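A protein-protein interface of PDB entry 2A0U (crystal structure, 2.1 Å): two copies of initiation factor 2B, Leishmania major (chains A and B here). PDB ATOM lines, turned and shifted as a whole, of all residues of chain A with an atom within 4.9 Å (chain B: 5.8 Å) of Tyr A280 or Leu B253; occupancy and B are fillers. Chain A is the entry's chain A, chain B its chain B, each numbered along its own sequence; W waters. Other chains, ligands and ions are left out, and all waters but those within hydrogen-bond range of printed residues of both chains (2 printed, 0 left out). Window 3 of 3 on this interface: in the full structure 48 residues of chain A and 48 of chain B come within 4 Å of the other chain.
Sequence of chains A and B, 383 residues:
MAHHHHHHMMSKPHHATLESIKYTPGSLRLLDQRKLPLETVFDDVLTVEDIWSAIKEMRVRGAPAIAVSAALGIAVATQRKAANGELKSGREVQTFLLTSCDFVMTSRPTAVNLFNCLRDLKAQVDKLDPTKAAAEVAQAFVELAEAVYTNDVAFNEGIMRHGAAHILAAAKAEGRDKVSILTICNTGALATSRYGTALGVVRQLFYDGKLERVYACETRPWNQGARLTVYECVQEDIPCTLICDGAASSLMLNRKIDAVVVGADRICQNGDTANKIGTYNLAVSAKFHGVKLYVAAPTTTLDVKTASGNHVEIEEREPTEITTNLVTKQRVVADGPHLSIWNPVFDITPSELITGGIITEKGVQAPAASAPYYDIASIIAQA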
ATOM      1  N   GLY A 278     -24.839  30.122   2.510  1.00  0.00           N
ATOM      2  CA  GLY A 278     -26.195  30.389   2.979  1.00  0.00           C
ATOM      3  C   GLY A 278     -27.266  30.067   1.949  1.00  0.00           C
ATOM      4  O   GLY A 278     -28.428  29.876   2.304  1.00  0.00           O
ATOM      5  N   THR A 279     -26.876  30.012   0.675  1.00  0.00           N
ATOM      6  CA  THR A 279     -27.813  29.721  -0.420  1.00  0.00           C
ATOM      7  C   THR A 279     -28.390  28.307  -0.312  1.00  0.00           C
ATOM      8  O   THR A 279     -29.585  28.098  -0.546  1.00  0.00           O
ATOM      9  CB  THR A 279     -27.161  29.923  -1.812  1.00  0.00           C
ATOM     10  OG1 THR A 279     -26.575  31.228  -1.884  1.00  0.00           O
ATOM     11  CG2 THR A 279     -28.192  29.781  -2.931  1.00  0.00           C
ATOM     12  N   TYR A 280     -27.539  27.348   0.044  1.00  0.00           N
ATOM     13  CA  TYR A 280     -27.969  25.969   0.267  1.00  0.00           C
ATOM     14  C   TYR A 280     -28.955  25.887   1.435  1.00  0.00           C
ATOM     15  O   TYR A 280     -29.977  25.205   1.345  1.00  0.00           O
ATOM     16  CB  TYR A 280     -26.752  25.068   0.511  1.00  0.00           C
ATOM     17  CG  TYR A 280     -27.070  23.620   0.824  1.00  0.00           C
ATOM     18  CD1 TYR A 280     -27.978  22.896   0.050  1.00  0.00           C
ATOM     19  CD2 TYR A 280     -26.434  22.964   1.880  1.00  0.00           C
ATOM     20  CE1 TYR A 280     -28.263  21.566   0.333  1.00  0.00           C
ATOM     21  CE2 TYR A 280     -26.709  21.631   2.168  1.00  0.00           C
ATOM     22  CZ  TYR A 280     -27.625  20.939   1.389  1.00  0.00           C
ATOM     23  OH  TYR A 280     -27.906  19.621   1.661  1.00  0.00           O
ATOM     24  N   ASN A 281     -28.635  26.597   2.516  1.00  0.00           N
ATOM     25  CA  ASN A 281     -29.507  26.720   3.685  1.00  0.00           C
ATOM     26  C   ASN A 281     -30.882  27.269   3.310  1.00  0.00           C
ATOM     27  O   ASN A 281     -31.910  26.792   3.797  1.00  0.00           O
ATOM     28  CB  ASN A 281     -28.840  27.626   4.729  1.00  0.00           C
ATOM     29  CG  ASN A 281     -29.458  27.499   6.110  1.00  0.00           C
ATOM     30  OD1 ASN A 281     -29.823  26.407   6.552  1.00  0.00           O
ATOM     31  ND2 ASN A 281     -29.561  28.622   6.809  1.00  0.00           N
ATOM     32  N   LEU A 282     -30.872  28.267   2.430  1.00  0.00           N
ATOM     33  CA  LEU A 282     -32.075  28.905   1.911  1.00  0.00           C
ATOM     34  C   LEU A 282     -32.895  27.928   1.061  1.00  0.00           C
ATOM     35  O   LEU A 282     -34.124  27.891   1.164  1.00  0.00           O
ATOM     36  CB  LEU A 282     -31.672  30.131   1.083  1.00  0.00           C
ATOM     37  CG  LEU A 282     -32.542  31.390   1.034  1.00  0.00           C
ATOM     38  CD1 LEU A 282     -32.809  31.946   2.429  1.00  0.00           C
ATOM     39  CD2 LEU A 282     -31.866  32.448   0.165  1.00  0.00           C
ATOM     40  N   ALA A 283     -32.199  27.140   0.240  1.00  0.00           N
ATOM     41  CA  ALA A 283     -32.818  26.145  -0.643  1.00  0.00           C
ATOM     42  C   ALA A 283     -33.490  25.004   0.121  1.00  0.00           C
ATOM     43  O   ALA A 283     -34.575  24.551  -0.258  1.00  0.00           O
ATOM     44  CB  ALA A 283     -31.788  25.593  -1.617  1.00  0.00           C
ATOM     45  N   VAL A 284     -32.836  24.541   1.186  1.00  0.00           N
ATOM     46  CA  VAL A 284     -33.382  23.502   2.058  1.00  0.00           C
ATOM     47  C   VAL A 284     -34.692  23.977   2.694  1.00  0.00           C
ATOM     48  O   VAL A 284     -35.682  23.238   2.720  1.00  0.00           O
ATOM     49  CB  VAL A 284     -32.356  23.077   3.150  1.00  0.00           C
ATOM     50  CG1 VAL A 284     -33.015  22.233   4.237  1.00  0.00           C
ATOM     51  CG2 VAL A 284     -31.188  22.322   2.527  1.00  0.00           C
ATOM     52  N   ASP A 347     -21.386  27.751  -0.942  1.00  0.00           N
ATOM     53  CA  ASP A 347     -21.859  26.378  -0.769  1.00  0.00           C
ATOM     54  C   ASP A 347     -22.524  25.891  -2.051  1.00  0.00           C
ATOM     55  O   ASP A 347     -22.687  26.664  -3.000  1.00  0.00           O
ATOM     56  CB  ASP A 347     -22.785  26.229   0.453  1.00  0.00           C
ATOM     57  CG  ASP A 347     -23.948  27.216   0.456  1.00  0.00           C
ATOM     58  OD1 ASP A 347     -24.482  27.551  -0.624  1.00  0.00           O
ATOM     59  OD2 ASP A 347     -24.346  27.641   1.564  1.00  0.00           O
ATOM     60  N   ILE A 348     -22.887  24.613  -2.084  1.00  0.00           N
ATOM     61  CA  ILE A 348     -23.532  24.039  -3.259  1.00  0.00           C
ATOM     62  C   ILE A 348     -25.020  23.824  -3.018  1.00  0.00           C
ATOM     63  O   ILE A 348     -25.423  23.237  -2.016  1.00  0.00           O
ATOM     64  CB  ILE A 348     -22.829  22.729  -3.740  1.00  0.00           C
ATOM     65  CG1 ILE A 348     -21.628  23.061  -4.627  1.00  0.00           C
ATOM     66  CG2 ILE A 348     -23.778  21.839  -4.536  1.00  0.00           C
ATOM     67  CD1 ILE A 348     -20.344  23.276  -3.879  1.00  0.00           C
ATOM     68  N   THR A 349     -25.826  24.343  -3.939  1.00  0.00           N
ATOM     69  CA  THR A 349     -27.244  24.034  -3.992  1.00  0.00           C
ATOM     70  C   THR A 349     -27.434  22.954  -5.059  1.00  0.00           C
ATOM     71  O   THR A 349     -27.248  23.222  -6.251  1.00  0.00           O
ATOM     72  CB  THR A 349     -28.091  25.290  -4.308  1.00  0.00           C
ATOM     73  OG1 THR A 349     -27.935  26.246  -3.253  1.00  0.00           O
ATOM     74  CG2 THR A 349     -29.568  24.937  -4.445  1.00  0.00           C
ATOM     75  N   PRO A 350     -27.783  21.724  -4.632  1.00  0.00           N
ATOM     76  CA  PRO A 350     -27.981  20.621  -5.574  1.00  0.00           C
ATOM     77  C   PRO A 350     -29.175  20.890  -6.481  1.00  0.00           C
ATOM     78  O   PRO A 350     -30.137  21.540  -6.058  1.00  0.00           O
ATOM     79  CB  PRO A 350     -28.263  19.421  -4.663  1.00  0.00           C
ATOM     80  CG  PRO A 350     -27.789  19.827  -3.306  1.00  0.00           C
ATOM     81  CD  PRO A 350     -28.015  21.300  -3.242  1.00  0.00           C
ATOM     82  N   LEU A 353     -32.953  20.927  -5.555  1.00  0.00           N
ATOM     83  CA  LEU A 353     -33.532  22.026  -4.777  1.00  0.00           C
ATOM     84  C   LEU A 353     -33.800  23.290  -5.603  1.00  0.00           C
ATOM     85  O   LEU A 353     -34.364  24.265  -5.093  1.00  0.00           O
ATOM     86  CB  LEU A 353     -32.648  22.343  -3.563  1.00  0.00           C
ATOM     87  CG  LEU A 353     -32.402  21.221  -2.545  1.00  0.00           C
ATOM     88  CD1 LEU A 353     -31.421  21.670  -1.480  1.00  0.00           C
ATOM     89  CD2 LEU A 353     -33.698  20.743  -1.901  1.00  0.00           C
ATOM     90  N   ALA B 248     -24.741  26.619   8.325  1.00  0.00           N
ATOM     91  CA  ALA B 248     -25.187  25.451   9.089  1.00  0.00           C
ATOM     92  C   ALA B 248     -25.595  24.254   8.224  1.00  0.00           C
ATOM     93  O   ALA B 248     -25.278  23.112   8.561  1.00  0.00           O
ATOM     94  CB  ALA B 248     -26.312  25.835  10.031  1.00  0.00           C
ATOM     95  N   SER B 249     -26.294  24.522   7.121  1.00  0.00           N
ATOM     96  CA  SER B 249     -26.724  23.468   6.197  1.00  0.00           C
ATOM     97  C   SER B 249     -25.546  22.805   5.491  1.00  0.00           C
ATOM     98  O   SER B 249     -25.490  21.577   5.388  1.00  0.00           O
ATOM     99  CB  SER B 249     -27.710  24.015   5.167  1.00  0.00           C
ATOM    100  OG  SER B 249     -29.011  24.116   5.714  1.00  0.00           O
ATOM    101  N   SER B 250     -24.613  23.626   5.008  1.00  0.00           N
ATOM    102  CA  SER B 250     -23.395  23.136   4.363  1.00  0.00           C
ATOM    103  C   SER B 250     -22.542  22.309   5.325  1.00  0.00           C
ATOM    104  O   SER B 250     -21.951  21.299   4.929  1.00  0.00           O
ATOM    105  CB  SER B 250     -22.576  24.300   3.805  1.00  0.00           C
ATOM    106  OG  SER B 250     -21.443  23.829   3.098  1.00  0.00           O
ATOM    107  N   LEU B 251     -22.485  22.743   6.585  1.00  0.00           N
ATOM    108  CA  LEU B 251     -21.754  22.021   7.625  1.00  0.00           C
ATOM    109  C   LEU B 251     -22.295  20.606   7.829  1.00  0.00           C
ATOM    110  O   LEU B 251     -21.524  19.644   7.861  1.00  0.00           O
ATOM    111  CB  LEU B 251     -21.775  22.795   8.951  1.00  0.00           C
ATOM    112  CG  LEU B 251     -21.049  22.157  10.147  1.00  0.00           C
ATOM    113  CD1 LEU B 251     -19.536  22.131   9.948  1.00  0.00           C
ATOM    114  CD2 LEU B 251     -21.410  22.862  11.442  1.00  0.00           C
ATOM    115  N   MET B 252     -23.617  20.492   7.954  1.00  0.00           N
ATOM    116  CA  MET B 252     -24.279  19.209   8.209  1.00  0.00           C
ATOM    117  C   MET B 252     -24.181  18.220   7.047  1.00  0.00           C
ATOM    118  O   MET B 252     -24.176  17.006   7.263  1.00  0.00           O
ATOM    119  CB  MET B 252     -25.742  19.426   8.606  1.00  0.00           C
ATOM    120  CG  MET B 252     -25.909  19.924  10.027  1.00  0.00           C
ATOM    121  SD  MET B 252     -27.762  20.047  10.611  1.00  0.00           S
ATOM    122  CE  MET B 252     -27.430  19.970  12.427  1.00  0.00           C
ATOM    123  N   LEU B 253     -24.106  18.741   5.823  1.00  0.00           N
ATOM    124  CA  LEU B 253     -23.945  17.898   4.640  1.00  0.00           C
ATOM    125  C   LEU B 253     -22.509  17.403   4.499  1.00  0.00           C
ATOM    126  O   LEU B 253     -22.276  16.225   4.221  1.00  0.00           O
ATOM    127  CB  LEU B 253     -24.366  18.643   3.367  1.00  0.00           C
ATOM    128  CG  LEU B 253     -24.271  17.854   2.053  1.00  0.00           C
ATOM    129  CD1 LEU B 253     -25.381  16.812   1.940  1.00  0.00           C
ATOM    130  CD2 LEU B 253     -24.292  18.788   0.860  1.00  0.00           C
ATOM    131  N   ASN B 254     -21.555  18.311   4.692  1.00  0.00           N
ATOM    132  CA  ASN B 254     -20.141  18.018   4.469  1.00  0.00           C
ATOM    133  C   ASN B 254     -19.438  17.304   5.624  1.00  0.00           C
ATOM    134  O   ASN B 254     -18.470  16.575   5.405  1.00  0.00           O
ATOM    135  CB  ASN B 254     -19.380  19.296   4.094  1.00  0.00           C
ATOM    136  CG  ASN B 254     -19.763  19.828   2.721  1.00  0.00           C
ATOM    137  OD1 ASN B 254     -20.159  20.986   2.580  1.00  0.00           O
ATOM    138  ND2 ASN B 254     -19.650  18.981   1.702  1.00  0.00           N
ATOM    139  N   ARG B 255     -19.919  17.522   6.846  1.00  0.00           N
ATOM    140  CA  ARG B 255     -19.312  16.915   8.032  1.00  0.00           C
ATOM    141  C   ARG B 255     -20.336  16.147   8.861  1.00  0.00           C
ATOM    142  O   ARG B 255     -21.530  16.455   8.829  1.00  0.00           O
ATOM    143  CB  ARG B 255     -18.618  17.973   8.898  1.00  0.00           C
ATOM    144  CG  ARG B 255     -17.444  18.679   8.224  1.00  0.00           C
ATOM    145  CD  ARG B 255     -16.686  19.561   9.204  1.00  0.00           C
ATOM    146  NE  ARG B 255     -15.754  20.465   8.528  1.00  0.00           N
ATOM    147  CZ  ARG B 255     -14.881  21.256   9.147  1.00  0.00           C
ATOM    148  NH1 ARG B 255     -14.082  22.041   8.437  1.00  0.00           N
ATOM    149  NH2 ARG B 255     -14.798  21.265  10.473  1.00  0.00           N
ATOM    150  N   PHE B 288     -33.650  17.621   7.465  1.00  0.00           N
ATOM    151  CA  PHE B 288     -33.228  17.364   6.086  1.00  0.00           C
ATOM    152  C   PHE B 288     -31.960  16.511   6.019  1.00  0.00           C
ATOM    153  O   PHE B 288     -31.825  15.663   5.134  1.00  0.00           O
ATOM    154  CB  PHE B 288     -33.018  18.686   5.337  1.00  0.00           C
ATOM    155  CG  PHE B 288     -32.671  18.520   3.877  1.00  0.00           C
ATOM    156  CD1 PHE B 288     -33.671  18.336   2.927  1.00  0.00           C
ATOM    157  CD2 PHE B 288     -31.345  18.567   3.452  1.00  0.00           C
ATOM    158  CE1 PHE B 288     -33.356  18.189   1.576  1.00  0.00           C
ATOM    159  CE2 PHE B 288     -31.019  18.420   2.103  1.00  0.00           C
ATOM    160  CZ  PHE B 288     -32.026  18.232   1.164  1.00  0.00           C
ATOM    161  N   HIS B 289     -31.045  16.743   6.958  1.00  0.00           N
ATOM    162  CA  HIS B 289     -29.741  16.073   6.977  1.00  0.00           C
ATOM    163  C   HIS B 289     -29.691  14.848   7.894  1.00  0.00           C
ATOM    164  O   HIS B 289     -28.646  14.205   8.020  1.00  0.00           O
ATOM    165  CB  HIS B 289     -28.642  17.066   7.366  1.00  0.00           C
ATOM    166  CG  HIS B 289     -28.432  18.156   6.363  1.00  0.00           C
ATOM    167  ND1 HIS B 289     -27.699  17.974   5.210  1.00  0.00           N
ATOM    168  CD2 HIS B 289     -28.861  19.440   6.338  1.00  0.00           C
ATOM    169  CE1 HIS B 289     -27.685  19.100   4.519  1.00  0.00           C
ATOM    170  NE2 HIS B 289     -28.382  20.005   5.181  1.00  0.00           N
HETATM  171  O   HOH W   1     -25.269  26.393   4.123  1.00  0.00           O
HETATM  172  O   HOH W   2     -22.319  22.789   0.606  1.00  0.00           O
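Tyr A280 touches just these residues of chain B: Ser B249 (3.4 Å), Ser B250 (3.7 Å), Leu B253 (3.8 Å), Phe B288 (3.4 Å) and His B289 (2.9 Å).
Leu B253 touches just one residue of chain A: Tyr A280 (3.8 Å).
Printed residues of chain A within 4 Å of Ser B249: Tyr A280 and Asn A281.
Printed residues of chain B within 4 Å of Asn A281: Ser B249 (2.6 Å).
Leu B251 touches none of the printed residues of chain A.
The nearest printed residue of chain A that does not touch Leu B253 is Ile A348 (5.4 Å).
The nearest printed residue of chain A that does not touch Ser B250 is Ile A348 (5.4 Å).
CE2 of Tyr A280 touches O of Ser B249, at 3.4 Å.
Ser B250 touches Tyr A280 (N to CD2, 3.7 Å).
OH of Tyr A280 touches CD1 of Leu B253, at 3.8 Å.
Tyr A280 touches Phe B288 (OH to CE2, 3.4 Å).
Tyr A280 touches His B289 (OH to CE1, 2.9 Å).
Val A284 touches Phe B288.
OG of Ser B250 touches CB of Asp A347, at 3.8 Å.
N of Gly A278 is in hydrogen-bond range of OD2 of Asp A347 (2.7 Å).
N of Tyr A280 sits at hydrogen-bond distance from OD1 of Asp A347 (3.1 Å).
The side-chain hydroxyl of Thr A349 sits at hydrogen-bond distance from the backbone NH of Tyr A280, 3.5 Å away.
O of Ser B249 is in hydrogen-bond range of NE2 of His B289, at 3.3 Å.
OD1 of Asn B254 sits close to O of Ser B250, 3.0 Å away.
No position is printed for both chains.
Water W2 lies within hydrogen-bond range of OG of Ser B250 (2.8 Å), N of Ile A348 (3.3 Å) and OD1 of Asn B254 (3.4 Å).
Water W1 lies within hydrogen-bond range of the backbone NH (N) of Ser B250 (3.0 Å) and the side-chain carboxylate (OD2) of Asp A347 (3.0 Å).
OG of Ser B249 lies within hydrogen-bond range of OD1 of Asn A281 (2.6 Å).
Hydrophobic or aromatic side chains of chain A within 4 Å of the printed part of chain B: Tyr A280 and Val A284.
Among the printed residues, no Asp or Glu carboxylate lies within 4 Å of a Lys or Arg side-chain nitrogen of the other chain.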
